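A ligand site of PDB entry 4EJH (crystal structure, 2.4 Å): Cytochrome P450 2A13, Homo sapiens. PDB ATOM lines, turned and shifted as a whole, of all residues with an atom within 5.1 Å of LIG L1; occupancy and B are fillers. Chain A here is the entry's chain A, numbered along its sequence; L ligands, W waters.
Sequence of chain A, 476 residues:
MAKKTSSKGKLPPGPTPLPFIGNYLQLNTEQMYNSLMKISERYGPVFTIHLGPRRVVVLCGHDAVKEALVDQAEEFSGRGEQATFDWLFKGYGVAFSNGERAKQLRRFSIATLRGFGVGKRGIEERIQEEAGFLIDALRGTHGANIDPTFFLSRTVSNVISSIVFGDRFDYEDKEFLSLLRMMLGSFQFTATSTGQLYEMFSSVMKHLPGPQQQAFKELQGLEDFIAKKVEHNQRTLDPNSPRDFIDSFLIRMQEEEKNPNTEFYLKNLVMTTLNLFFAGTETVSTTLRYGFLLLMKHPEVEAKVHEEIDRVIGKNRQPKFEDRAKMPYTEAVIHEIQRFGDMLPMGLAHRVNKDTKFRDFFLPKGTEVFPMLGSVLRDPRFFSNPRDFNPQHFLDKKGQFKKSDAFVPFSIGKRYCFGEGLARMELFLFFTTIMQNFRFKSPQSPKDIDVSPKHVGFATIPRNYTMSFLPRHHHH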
ATOM      1  N   LEU A  69      10.463  -8.596  -3.919  1.00  0.00           N
ATOM      2  CA  LEU A  69      11.103  -8.154  -2.673  1.00  0.00           C
ATOM      3  C   LEU A  69      12.484  -7.504  -2.894  1.00  0.00           C
ATOM      4  O   LEU A  69      12.886  -6.675  -2.113  1.00  0.00           O
ATOM      5  CB  LEU A  69      11.254  -9.304  -1.698  1.00  0.00           C
ATOM      6  CG  LEU A  69      10.084  -9.771  -0.815  1.00  0.00           C
ATOM      7  CD1 LEU A  69       8.823 -10.297  -1.606  1.00  0.00           C
ATOM      8  CD2 LEU A  69      10.630 -10.926   0.000  1.00  0.00           C
ATOM      9  N   ARG A  79       4.888  -4.597   6.274  1.00  0.00           N
ATOM     10  CA  ARG A  79       4.676  -5.852   6.982  1.00  0.00           C
ATOM     11  C   ARG A  79       3.229  -6.169   6.955  1.00  0.00           C
ATOM     12  O   ARG A  79       2.393  -5.343   7.320  1.00  0.00           O
ATOM     13  CB  ARG A  79       5.178  -5.793   8.435  1.00  0.00           C
ATOM     14  CG  ARG A  79       4.731  -6.984   9.411  1.00  0.00           C
ATOM     15  CD  ARG A  79       5.449  -8.319   9.162  1.00  0.00           C
ATOM     16  NE  ARG A  79       6.898  -8.215   9.154  1.00  0.00           N
ATOM     17  CZ  ARG A  79       7.721  -8.738   8.261  1.00  0.00           C
ATOM     18  NH1 ARG A  79       7.252  -9.428   7.211  1.00  0.00           N
ATOM     19  NH2 ARG A  79       9.019  -8.601   8.438  1.00  0.00           N
ATOM     20  N   VAL A  94       9.848  -4.492  16.456  1.00  0.00           N
ATOM     21  CA  VAL A  94      10.558  -4.310  15.227  1.00  0.00           C
ATOM     22  C   VAL A  94       9.900  -5.160  14.140  1.00  0.00           C
ATOM     23  O   VAL A  94       9.647  -4.691  13.049  1.00  0.00           O
ATOM     24  CB  VAL A  94      12.065  -4.662  15.442  1.00  0.00           C
ATOM     25  CG1 VAL A  94      12.272  -6.236  15.763  1.00  0.00           C
ATOM     26  CG2 VAL A  94      12.917  -4.188  14.267  1.00  0.00           C
ATOM     27  N   ALA A  95       9.583  -6.413  14.473  1.00  0.00           N
ATOM     28  CA  ALA A  95       9.087  -7.397  13.489  1.00  0.00           C
ATOM     29  C   ALA A  95       7.638  -7.176  13.002  1.00  0.00           C
ATOM     30  O   ALA A  95       7.327  -7.545  11.878  1.00  0.00           O
ATOM     31  CB  ALA A  95       9.251  -8.794  14.050  1.00  0.00           C
ATOM     32  N   ARG A 106      14.242  -1.154  13.359  1.00  0.00           N
ATOM     33  CA  ARG A 106      15.212  -2.001  12.646  1.00  0.00           C
ATOM     34  C   ARG A 106      16.612  -1.375  12.623  1.00  0.00           C
ATOM     35  O   ARG A 106      17.620  -2.008  12.956  1.00  0.00           O
ATOM     36  CB  ARG A 106      14.720  -2.293  11.207  1.00  0.00           C
ATOM     37  CG  ARG A 106      15.461  -3.350  10.494  1.00  0.00           C
ATOM     38  CD  ARG A 106      14.838  -3.598   9.077  1.00  0.00           C
ATOM     39  NE  ARG A 106      15.828  -4.337   8.322  1.00  0.00           N
ATOM     40  CZ  ARG A 106      15.800  -5.652   8.099  1.00  0.00           C
ATOM     41  NH1 ARG A 106      14.791  -6.438   8.529  1.00  0.00           N
ATOM     42  NH2 ARG A 106      16.764  -6.194   7.384  1.00  0.00           N
ATOM     43  N   LEU A 113      22.733  -4.637  18.174  1.00  0.00           N
ATOM     44  CA  LEU A 113      23.162  -6.034  17.996  1.00  0.00           C
ATOM     45  C   LEU A 113      24.581  -6.202  17.461  1.00  0.00           C
ATOM     46  O   LEU A 113      25.366  -6.912  18.083  1.00  0.00           O
ATOM     47  CB  LEU A 113      22.148  -6.761  17.124  1.00  0.00           C
ATOM     48  CG  LEU A 113      21.153  -7.706  17.798  1.00  0.00           C
ATOM     49  CD1 LEU A 113      20.940  -7.601  19.278  1.00  0.00           C
ATOM     50  CD2 LEU A 113      19.834  -7.855  17.011  1.00  0.00           C
ATOM     51  N   ILE A 160      21.042 -15.741  22.778  1.00  0.00           N
ATOM     52  CA  ILE A 160      20.350 -14.457  22.630  1.00  0.00           C
ATOM     53  C   ILE A 160      20.026 -13.890  23.986  1.00  0.00           C
ATOM     54  O   ILE A 160      19.933 -12.658  24.120  1.00  0.00           O
ATOM     55  CB  ILE A 160      19.081 -14.499  21.701  1.00  0.00           C
ATOM     56  CG1 ILE A 160      18.445 -13.121  21.497  1.00  0.00           C
ATOM     57  CG2 ILE A 160      17.977 -15.392  22.304  1.00  0.00           C
ATOM     58  CD1 ILE A 160      19.213 -12.167  20.705  1.00  0.00           C
ATOM     59  N   ASN A 275      10.531  -9.933  20.373  1.00  0.00           N
ATOM     60  CA  ASN A 275      10.867 -10.364  18.999  1.00  0.00           C
ATOM     61  C   ASN A 275      12.205 -11.047  18.935  1.00  0.00           C
ATOM     62  O   ASN A 275      12.354 -12.096  18.295  1.00  0.00           O
ATOM     63  CB  ASN A 275      10.886  -9.207  17.929  1.00  0.00           C
ATOM     64  CG  ASN A 275       9.559  -8.583  17.717  1.00  0.00           C
ATOM     65  OD1 ASN A 275       9.444  -7.371  17.465  1.00  0.00           O
ATOM     66  ND2 ASN A 275       8.512  -9.393  17.786  1.00  0.00           N
ATOM     67  N   LEU A 276      13.225 -10.453  19.575  1.00  0.00           N
ATOM     68  CA  LEU A 276      14.560 -11.002  19.460  1.00  0.00           C
ATOM     69  C   LEU A 276      14.737 -12.263  20.278  1.00  0.00           C
ATOM     70  O   LEU A 276      15.500 -13.124  19.885  1.00  0.00           O
ATOM     71  CB  LEU A 276      15.621  -9.962  19.878  1.00  0.00           C
ATOM     72  CG  LEU A 276      15.587  -8.673  19.094  1.00  0.00           C
ATOM     73  CD1 LEU A 276      16.494  -7.656  19.828  1.00  0.00           C
ATOM     74  CD2 LEU A 276      16.031  -9.018  17.659  1.00  0.00           C
ATOM     75  N   ALA A 279      12.383 -15.088  18.413  1.00  0.00           N
ATOM     76  CA  ALA A 279      13.012 -15.575  17.141  1.00  0.00           C
ATOM     77  C   ALA A 279      14.427 -16.078  17.334  1.00  0.00           C
ATOM     78  O   ALA A 279      14.815 -17.024  16.633  1.00  0.00           O
ATOM     79  CB  ALA A 279      12.975 -14.489  16.048  1.00  0.00           C
ATOM     80  N   GLY A 280      15.195 -15.454  18.261  1.00  0.00           N
ATOM     81  CA  GLY A 280      16.528 -15.907  18.565  1.00  0.00           C
ATOM     82  C   GLY A 280      16.523 -17.243  19.293  1.00  0.00           C
ATOM     83  O   GLY A 280      17.561 -17.854  19.482  1.00  0.00           O
ATOM     84  N   THR A 283      13.622 -20.635  15.945  1.00  0.00           N
ATOM     85  CA  THR A 283      13.960 -21.118  14.601  1.00  0.00           C
ATOM     86  C   THR A 283      15.212 -21.981  14.513  1.00  0.00           C
ATOM     87  O   THR A 283      15.163 -23.052  13.924  1.00  0.00           O
ATOM     88  CB  THR A 283      14.099 -20.007  13.526  1.00  0.00           C
ATOM     89  OG1 THR A 283      14.905 -18.942  14.051  1.00  0.00           O
ATOM     90  CG2 THR A 283      12.729 -19.495  13.078  1.00  0.00           C
ATOM     91  N   VAL A 284      16.320 -21.476  15.026  1.00  0.00           N
ATOM     92  CA  VAL A 284      17.595 -22.209  15.128  1.00  0.00           C
ATOM     93  C   VAL A 284      17.389 -23.527  15.900  1.00  0.00           C
ATOM     94  O   VAL A 284      17.696 -24.579  15.406  1.00  0.00           O
ATOM     95  CB  VAL A 284      18.696 -21.333  15.770  1.00  0.00           C
ATOM     96  CG1 VAL A 284      19.975 -22.114  16.081  1.00  0.00           C
ATOM     97  CG2 VAL A 284      19.040 -20.134  14.838  1.00  0.00           C
ATOM     98  N   THR A 287      15.514 -25.914  13.716  1.00  0.00           N
ATOM     99  CA  THR A 287      16.368 -26.310  12.612  1.00  0.00           C
ATOM    100  C   THR A 287      17.373 -27.386  13.037  1.00  0.00           C
ATOM    101  O   THR A 287      17.653 -28.323  12.295  1.00  0.00           O
ATOM    102  CB  THR A 287      17.070 -25.102  12.036  1.00  0.00           C
ATOM    103  OG1 THR A 287      16.072 -24.149  11.655  1.00  0.00           O
ATOM    104  CG2 THR A 287      17.896 -25.469  10.801  1.00  0.00           C
ATOM    105  N   GLN A 338      18.496 -26.567   6.065  1.00  0.00           N
ATOM    106  CA  GLN A 338      17.646 -25.354   6.105  1.00  0.00           C
ATOM    107  C   GLN A 338      16.668 -25.347   4.937  1.00  0.00           C
ATOM    108  O   GLN A 338      15.504 -24.959   5.096  1.00  0.00           O
ATOM    109  CB  GLN A 338      18.499 -24.094   6.060  1.00  0.00           C
ATOM    110  CG  GLN A 338      19.122 -23.822   7.398  1.00  0.00           C
ATOM    111  CD  GLN A 338      19.619 -22.388   7.553  1.00  0.00           C
ATOM    112  OE1 GLN A 338      20.758 -22.079   7.185  1.00  0.00           O
ATOM    113  NE2 GLN A 338      18.764 -21.511   8.082  1.00  0.00           N
ATOM    114  N   MET A 343      11.497 -23.662   7.132  1.00  0.00           N
ATOM    115  CA  MET A 343      11.089 -23.295   8.450  1.00  0.00           C
ATOM    116  C   MET A 343       9.885 -22.336   8.417  1.00  0.00           C
ATOM    117  O   MET A 343       8.874 -22.510   9.162  1.00  0.00           O
ATOM    118  CB  MET A 343      12.316 -22.658   9.095  1.00  0.00           C
ATOM    119  CG  MET A 343      12.250 -22.318  10.562  1.00  0.00           C
ATOM    120  SD  MET A 343      12.444 -23.787  11.558  1.00  0.00           S
ATOM    121  CE  MET A 343      10.646 -23.907  11.976  1.00  0.00           C
ATOM    122  N   LEU A 344       9.954 -21.349   7.540  1.00  0.00           N
ATOM    123  CA  LEU A 344       8.841 -20.457   7.351  1.00  0.00           C
ATOM    124  C   LEU A 344       8.343 -20.505   5.926  1.00  0.00           C
ATOM    125  O   LEU A 344       8.804 -19.756   5.087  1.00  0.00           O
ATOM    126  CB  LEU A 344       9.220 -19.036   7.763  1.00  0.00           C
ATOM    127  CG  LEU A 344       9.584 -18.678   9.216  1.00  0.00           C
ATOM    128  CD1 LEU A 344       9.591 -17.187   9.253  1.00  0.00           C
ATOM    129  CD2 LEU A 344       8.580 -19.187  10.207  1.00  0.00           C
ATOM    130  N   GLY A 347       7.170 -17.242   4.544  1.00  0.00           N
ATOM    131  CA  GLY A 347       7.778 -16.249   5.373  1.00  0.00           C
ATOM    132  C   GLY A 347       6.807 -15.533   6.291  1.00  0.00           C
ATOM    133  O   GLY A 347       5.772 -16.036   6.681  1.00  0.00           O
ATOM    134  N   LEU A 348       7.166 -14.307   6.622  1.00  0.00           N
ATOM    135  CA  LEU A 348       6.295 -13.397   7.277  1.00  0.00           C
ATOM    136  C   LEU A 348       5.595 -12.601   6.187  1.00  0.00           C
ATOM    137  O   LEU A 348       6.249 -12.184   5.200  1.00  0.00           O
ATOM    138  CB  LEU A 348       7.221 -12.469   8.044  1.00  0.00           C
ATOM    139  CG  LEU A 348       6.742 -12.035   9.377  1.00  0.00           C
ATOM    140  CD1 LEU A 348       5.703 -13.073   9.830  1.00  0.00           C
ATOM    141  CD2 LEU A 348       7.902 -11.874  10.330  1.00  0.00           C
ATOM    142  N   HIS A 350       4.162  -9.800   4.019  1.00  0.00           N
ATOM    143  CA  HIS A 350       4.327  -8.405   3.675  1.00  0.00           C
ATOM    144  C   HIS A 350       3.042  -7.735   3.294  1.00  0.00           C
ATOM    145  O   HIS A 350       1.964  -8.364   3.267  1.00  0.00           O
ATOM    146  CB  HIS A 350       5.241  -8.263   2.460  1.00  0.00           C
ATOM    147  CG  HIS A 350       6.648  -8.637   2.704  1.00  0.00           C
ATOM    148  ND1 HIS A 350       7.690  -7.779   2.425  1.00  0.00           N
ATOM    149  CD2 HIS A 350       7.197  -9.750   3.243  1.00  0.00           C
ATOM    150  CE1 HIS A 350       8.831  -8.355   2.780  1.00  0.00           C
ATOM    151  NE2 HIS A 350       8.564  -9.552   3.260  1.00  0.00           N
ATOM    152  N   LEU A 373       8.414 -18.535   0.357  1.00  0.00           N
ATOM    153  CA  LEU A 373       9.838 -18.939   0.416  1.00  0.00           C
ATOM    154  C   LEU A 373      10.014 -20.440   0.266  1.00  0.00           C
ATOM    155  O   LEU A 373      10.997 -20.912  -0.294  1.00  0.00           O
ATOM    156  CB  LEU A 373      10.438 -18.448   1.765  1.00  0.00           C
ATOM    157  CG  LEU A 373      10.259 -16.935   2.118  1.00  0.00           C
ATOM    158  CD1 LEU A 373      10.935 -16.632   3.459  1.00  0.00           C
ATOM    159  CD2 LEU A 373      10.867 -15.994   1.058  1.00  0.00           C
ATOM    160  N   PRO A 409      15.999 -18.961   2.864  1.00  0.00           N
ATOM    161  CA  PRO A 409      15.231 -19.206   4.106  1.00  0.00           C
ATOM    162  C   PRO A 409      15.070 -18.030   5.081  1.00  0.00           C
ATOM    163  O   PRO A 409      14.095 -18.004   5.881  1.00  0.00           O
ATOM    164  CB  PRO A 409      16.022 -20.325   4.759  1.00  0.00           C
ATOM    165  CG  PRO A 409      17.423 -19.963   4.419  1.00  0.00           C
ATOM    166  CD  PRO A 409      17.331 -19.579   2.938  1.00  0.00           C
ATOM    167  N   PHE A 410      15.989 -17.052   5.031  1.00  0.00           N
ATOM    168  CA  PHE A 410      15.920 -15.788   5.804  1.00  0.00           C
ATOM    169  C   PHE A 410      15.224 -14.656   5.057  1.00  0.00           C
ATOM    170  O   PHE A 410      15.352 -13.459   5.419  1.00  0.00           O
ATOM    171  CB  PHE A 410      17.312 -15.302   6.182  1.00  0.00           C
ATOM    172  CG  PHE A 410      18.110 -16.298   6.883  1.00  0.00           C
ATOM    173  CD1 PHE A 410      17.853 -16.596   8.245  1.00  0.00           C
ATOM    174  CD2 PHE A 410      19.107 -16.987   6.213  1.00  0.00           C
ATOM    175  CE1 PHE A 410      18.588 -17.553   8.902  1.00  0.00           C
ATOM    176  CE2 PHE A 410      19.841 -17.965   6.877  1.00  0.00           C
ATOM    177  CZ  PHE A 410      19.578 -18.222   8.219  1.00  0.00           C
ATOM    178  N   SER A 411      14.490 -15.013   4.005  1.00  0.00           N
ATOM    179  CA  SER A 411      13.841 -14.050   3.105  1.00  0.00           C
ATOM    180  C   SER A 411      14.880 -13.085   2.413  1.00  0.00           C
ATOM    181  O   SER A 411      16.050 -13.346   2.433  1.00  0.00           O
ATOM    182  CB  SER A 411      12.679 -13.384   3.775  1.00  0.00           C
ATOM    183  OG  SER A 411      12.033 -12.474   2.940  1.00  0.00           O
ATOM    184  N   ILE A 412      14.420 -12.031   1.753  1.00  0.00           N
ATOM    185  CA  ILE A 412      15.331 -11.222   0.968  1.00  0.00           C
ATOM    186  C   ILE A 412      14.678  -9.813   0.949  1.00  0.00           C
ATOM    187  O   ILE A 412      13.517  -9.657   1.333  1.00  0.00           O
ATOM    188  CB  ILE A 412      15.481 -11.790  -0.509  1.00  0.00           C
ATOM    189  CG1 ILE A 412      14.112 -12.202  -1.110  1.00  0.00           C
ATOM    190  CG2 ILE A 412      16.511 -12.933  -0.603  1.00  0.00           C
ATOM    191  CD1 ILE A 412      14.167 -12.644  -2.624  1.00  0.00           C
ATOM    192  N   ARG A 415      13.181  -6.182   4.342  1.00  0.00           N
ATOM    193  CA  ARG A 415      12.855  -6.708   5.670  1.00  0.00           C
ATOM    194  C   ARG A 415      13.458  -8.075   5.939  1.00  0.00           C
ATOM    195  O   ARG A 415      12.919  -8.819   6.765  1.00  0.00           O
ATOM    196  CB  ARG A 415      11.353  -6.781   5.935  1.00  0.00           C
ATOM    197  CG  ARG A 415      10.578  -5.493   5.748  1.00  0.00           C
ATOM    198  CD  ARG A 415      10.714  -4.496   6.891  1.00  0.00           C
ATOM    199  NE  ARG A 415      10.130  -4.960   8.152  1.00  0.00           N
ATOM    200  CZ  ARG A 415       9.042  -4.458   8.698  1.00  0.00           C
ATOM    201  NH1 ARG A 415       8.598  -4.920   9.856  1.00  0.00           N
ATOM    202  NH2 ARG A 415       8.360  -3.492   8.088  1.00  0.00           N
ATOM    203  N   TYR A 416      14.553  -8.397   5.259  1.00  0.00           N
ATOM    204  CA  TYR A 416      15.153  -9.708   5.369  1.00  0.00           C
ATOM    205  C   TYR A 416      15.489  -9.919   6.853  1.00  0.00           C
ATOM    206  O   TYR A 416      15.624  -8.918   7.590  1.00  0.00           O
ATOM    207  CB  TYR A 416      16.381  -9.859   4.419  1.00  0.00           C
ATOM    208  CG  TYR A 416      17.663  -9.301   5.002  1.00  0.00           C
ATOM    209  CD1 TYR A 416      18.548 -10.135   5.654  1.00  0.00           C
ATOM    210  CD2 TYR A 416      17.952  -7.932   4.957  1.00  0.00           C
ATOM    211  CE1 TYR A 416      19.740  -9.636   6.243  1.00  0.00           C
ATOM    212  CE2 TYR A 416      19.105  -7.420   5.511  1.00  0.00           C
ATOM    213  CZ  TYR A 416      20.001  -8.293   6.175  1.00  0.00           C
ATOM    214  OH  TYR A 416      21.187  -7.847   6.787  1.00  0.00           O
ATOM    215  N   CYS A 417      15.624 -11.184   7.275  1.00  0.00           N
ATOM    216  CA  CYS A 417      15.931 -11.521   8.672  1.00  0.00           C
ATOM    217  C   CYS A 417      17.285 -10.993   9.080  1.00  0.00           C
ATOM    218  O   CYS A 417      18.307 -11.544   8.686  1.00  0.00           O
ATOM    219  CB  CYS A 417      16.005 -13.046   8.870  1.00  0.00           C
ATOM    220  SG  CYS A 417      16.456 -13.600  10.607  1.00  0.00           S
ATOM    221  N   PHE A 418      17.323  -9.985   9.926  1.00  0.00           N
ATOM    222  CA  PHE A 418      18.601  -9.544  10.344  1.00  0.00           C
ATOM    223  C   PHE A 418      19.192 -10.444  11.444  1.00  0.00           C
ATOM    224  O   PHE A 418      20.294 -10.185  11.924  1.00  0.00           O
ATOM    225  CB  PHE A 418      18.578  -8.048  10.649  1.00  0.00           C
ATOM    226  CG  PHE A 418      17.730  -7.663  11.802  1.00  0.00           C
ATOM    227  CD1 PHE A 418      18.164  -7.879  13.120  1.00  0.00           C
ATOM    228  CD2 PHE A 418      16.496  -7.050  11.598  1.00  0.00           C
ATOM    229  CE1 PHE A 418      17.347  -7.495  14.209  1.00  0.00           C
ATOM    230  CE2 PHE A 418      15.685  -6.604  12.678  1.00  0.00           C
ATOM    231  CZ  PHE A 418      16.080  -6.837  13.969  1.00  0.00           C
ATOM    232  N   GLY A 419      18.510 -11.517  11.805  1.00  0.00           N
ATOM    233  CA  GLY A 419      19.177 -12.527  12.673  1.00  0.00           C
ATOM    234  C   GLY A 419      20.115 -13.459  11.902  1.00  0.00           C
ATOM    235  O   GLY A 419      20.764 -14.379  12.475  1.00  0.00           O
ATOM    236  N   LEU A 422      23.623 -14.101  13.091  1.00  0.00           N
ATOM    237  CA  LEU A 422      23.681 -14.910  14.279  1.00  0.00           C
ATOM    238  C   LEU A 422      23.341 -16.360  14.017  1.00  0.00           C
ATOM    239  O   LEU A 422      23.950 -17.277  14.578  1.00  0.00           O
ATOM    240  CB  LEU A 422      22.777 -14.351  15.378  1.00  0.00           C
ATOM    241  CG  LEU A 422      22.968 -15.137  16.688  1.00  0.00           C
ATOM    242  CD1 LEU A 422      24.459 -14.926  17.308  1.00  0.00           C
ATOM    243  CD2 LEU A 422      21.923 -14.796  17.676  1.00  0.00           C
ATOM    244  N   ALA A 423      22.327 -16.588  13.191  1.00  0.00           N
ATOM    245  CA  ALA A 423      21.862 -17.940  12.927  1.00  0.00           C
ATOM    246  C   ALA A 423      22.948 -18.784  12.239  1.00  0.00           C
ATOM    247  O   ALA A 423      23.276 -19.870  12.740  1.00  0.00           O
ATOM    248  CB  ALA A 423      20.626 -17.888  12.105  1.00  0.00           C
ATOM    249  N   LEU A 427      24.256 -22.061  13.881  1.00  0.00           N
ATOM    250  CA  LEU A 427      24.082 -23.381  13.256  1.00  0.00           C
ATOM    251  C   LEU A 427      25.401 -24.089  12.950  1.00  0.00           C
ATOM    252  O   LEU A 427      25.561 -25.273  13.235  1.00  0.00           O
ATOM    253  CB  LEU A 427      23.240 -23.312  11.992  1.00  0.00           C
ATOM    254  CG  LEU A 427      21.779 -23.009  12.238  1.00  0.00           C
ATOM    255  CD1 LEU A 427      21.228 -22.529  10.879  1.00  0.00           C
ATOM    256  CD2 LEU A 427      21.039 -24.235  12.823  1.00  0.00           C
HETATM  257  C1  LIG L   1      12.330 -11.929  10.190  1.00  0.00           C
HETATM  258  C2  LIG L   1      13.764 -16.422   9.258  1.00  0.00           C
HETATM  259  C3  LIG L   1      16.679 -16.556  13.006  1.00  0.00           C
HETATM  260  C4  LIG L   1      15.039 -12.198  14.216  1.00  0.00           C
HETATM  261  C5  LIG L   1      12.468 -13.145   9.575  1.00  0.00           C
HETATM  262  C6  LIG L   1      11.876 -13.557   8.340  1.00  0.00           C
HETATM  263  C7  LIG L   1      12.323 -14.783   8.070  1.00  0.00           C
HETATM  264  C8  LIG L   1      13.174 -15.190   9.153  1.00  0.00           C
HETATM  265  C9  LIG L   1      11.976 -15.687   6.836  1.00  0.00           C
HETATM  266  C10 LIG L   1      10.952 -12.703   7.465  1.00  0.00           C
HETATM  267  C11 LIG L   1      11.681 -11.702   6.574  1.00  0.00           C
HETATM  268  C12 LIG L   1      10.589 -10.959   5.838  1.00  0.00           C
HETATM  269  O1  LIG L   1      10.585 -10.954   4.586  1.00  0.00           O
HETATM  270  O2  LIG L   1       9.679 -10.352   6.453  1.00  0.00           O
HETATM  271  C13 LIG L   1      14.626 -16.902  10.180  1.00  0.00           C
HETATM  272  C14 LIG L   1      15.239 -18.217  10.178  1.00  0.00           C
HETATM  273  C15 LIG L   1      16.085 -18.225  11.216  1.00  0.00           C
HETATM  274  C16 LIG L   1      15.976 -16.945  11.896  1.00  0.00           C
HETATM  275  C17 LIG L   1      14.965 -19.358   9.139  1.00  0.00           C
HETATM  276  C18 LIG L   1      16.950 -19.375  11.744  1.00  0.00           C
HETATM  277  C19 LIG L   1      17.446 -20.316  10.969  1.00  0.00           C
HETATM  278  C20 LIG L   1      16.535 -15.353  13.651  1.00  0.00           C
HETATM  279  C21 LIG L   1      17.295 -14.923  14.791  1.00  0.00           C
HETATM  280  C22 LIG L   1      16.856 -13.718  15.110  1.00  0.00           C
HETATM  281  C23 LIG L   1      15.775 -13.365  14.208  1.00  0.00           C
HETATM  282  C24 LIG L   1      18.443 -15.714  15.472  1.00  0.00           C
HETATM  283  C25 LIG L   1      17.397 -12.896  16.310  1.00  0.00           C
HETATM  284  C26 LIG L   1      18.398 -12.038  16.076  1.00  0.00           C
HETATM  285  C27 LIG L   1      14.186 -11.736  13.285  1.00  0.00           C
HETATM  286  C28 LIG L   1      13.504 -10.438  13.360  1.00  0.00           C
HETATM  287  C29 LIG L   1      12.664 -10.349  12.089  1.00  0.00           C
HETATM  288  C30 LIG L   1      12.903 -11.592  11.401  1.00  0.00           C
HETATM  289  C31 LIG L   1      13.625  -9.383  14.491  1.00  0.00           C
HETATM  290  C32 LIG L   1      11.769  -9.217  11.611  1.00  0.00           C
HETATM  291  C33 LIG L   1      12.500  -8.365  10.589  1.00  0.00           C
HETATM  292  C34 LIG L   1      11.722  -7.121  10.215  1.00  0.00           C
HETATM  293  O3  LIG L   1      12.317  -6.103   9.743  1.00  0.00           O
HETATM  294  O4  LIG L   1      10.492  -7.093  10.369  1.00  0.00           O
HETATM  295  N1  LIG L   1      13.269 -14.162  10.037  1.00  0.00           N
HETATM  296  N2  LIG L   1      15.088 -16.152  11.224  1.00  0.00           N
HETATM  297  N3  LIG L   1      15.648 -14.389  13.317  1.00  0.00           N
HETATM  298  N4  LIG L   1      13.784 -12.377  12.118  1.00  0.00           N
HETATM  299 FE1  LIG L   1      14.466 -14.282  11.621  1.00  0.00          FE
HETATM  300  O1  LG2 L   2      13.283 -16.059  13.017  1.00  0.00           O
HETATM  301  N1  LG2 L   2      12.221 -15.436  12.934  1.00  0.00           N
HETATM  302  N2  LG2 L   2      11.020 -16.071  13.210  1.00  0.00           N
HETATM  303  C1  LG2 L   2      10.897 -16.770  14.553  1.00  0.00           C
HETATM  304  C2  LG2 L   2      10.155 -14.910  13.196  1.00  0.00           C
HETATM  305  C3  LG2 L   2       8.664 -15.340  13.230  1.00  0.00           C
HETATM  306  C4  LG2 L   2       7.972 -13.984  13.321  1.00  0.00           C
HETATM  307  C5  LG2 L   2       8.803 -13.185  14.269  1.00  0.00           C
HETATM  308  O2  LG2 L   2       9.777 -12.541  13.876  1.00  0.00           O
HETATM  309  C6  LG2 L   2       8.405 -13.188  15.710  1.00  0.00           C
HETATM  310  C7  LG2 L   2       7.266 -13.867  16.125  1.00  0.00           C
HETATM  311  C8  LG2 L   2       6.911 -13.827  17.469  1.00  0.00           C
HETATM  312  C9  LG2 L   2       7.700 -13.105  18.355  1.00  0.00           C
HETATM  313  N3  LG2 L   2       8.791 -12.456  17.929  1.00  0.00           N
HETATM  314  C10 LG2 L   2       9.159 -12.475  16.632  1.00  0.00           C
HETATM  315  O   HOH W   1      16.278 -22.622   8.847  1.00  0.00           O
HETATM  316  O   HOH W   2       8.771 -13.136   4.342  1.00  0.00           O
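The side-chain hydroxyl (OG) of Ser 411 sits at hydrogen-bond distance from an oxygen (O1) of LIG L1, 2.7 Å away.
The guanidinium group (NH1) of Arg 79 is in salt-bridge range of an oxygen (O2) of LIG L1 (2.7 Å).
N3 of LG2 L2 lies within hydrogen-bond range of ND2 of Asn 275, at 3.1 Å.
An iron atom (FE1) of LIG L1 is bound by the side-chain sulfur of Cys 417 (2.3 Å).
NH1 of Arg 106 lies within salt-bridge range of O3 of LIG L1 (2.8 Å).
An oxygen (O1) of LIG L1 is in hydrogen-bond range of a ring nitrogen (NE2) of His 350 (2.8 Å).
OG1 of Thr 283 lies close to O1 of LG2 L2 (3.5 Å).
NH1 of Arg 415 lies within salt-bridge range of O4 of LIG L1, 2.9 Å away.
O1 of LG2 L2 binds FE1 of LIG L1 (2.6 Å).
N of Cys 417 sits at hydrogen-bond distance from O of Phe 410 (2.9 Å).
OG1 of Thr 283 is in hydrogen-bond range of O of Ala 279 (3.2 Å).
The side-chain amide oxygen (OD1) of Asn 275 is in hydrogen-bond range of the backbone NH (N) of Val 94.
The side-chain amide oxygen (OD1) of Asn 275 sits at hydrogen-bond distance from the backbone NH (N) of Ala 95 (3.1 Å).
NH1 of Arg 415 sits at hydrogen-bond distance from O of Val 94, 3.4 Å away.
The guanidinium group of Arg 106 is in hydrogen-bond range of the backbone carbonyl oxygen of Tyr 416 (2.8 Å).
The side-chain hydroxyl (OG1) of Thr 287 is in hydrogen-bond range of the backbone carbonyl oxygen (O) of Thr 283 (2.7 Å).
The side-chain sulfur (SG) of Cys 417 sits close to the backbone NH (N) of Gly 419, at 3.2 Å.
Residues that only touch LIG L1: Val 94 (3.7 Å), Ala 95 (3.4 Å), Leu 276 (3.99 Å), Ala 279 (3.5 Å), Gly 280 (3.6 Å), Thr 283 (3.1 Å), Val 284 (3.8 Å), Gln 338 (3.4 Å), Leu 344 (3.7 Å), Leu 348 (3.6 Å), Leu 373 (3.7 Å), Pro 409 (3.3 Å), Phe 410 (3.5 Å), Phe 418 (3.6 Å), Gly 419 (3.5 Å) and Ala 423 (3.98 Å).
Hydrophobic or aromatic side chains within 4 Å of LIG L1: Val 94, Ala 95, Leu 276, Ala 279, Val 284, Leu 344, Leu 348, His 350, Leu 373, Phe 410, Phe 418 and Ala 423.
The nearest printed residue that does not touch LIG L1 is Thr 287 (4.1 Å).
Water W2 lies within hydrogen-bond range of the backbone carbonyl oxygen of Leu 348 (2.8 Å) and an oxygen (O1) of LIG L1 (2.8 Å).
Water W1 lies within hydrogen-bond range of the side-chain amide nitrogen of Gln 338 and the side-chain hydroxyl of Thr 287.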
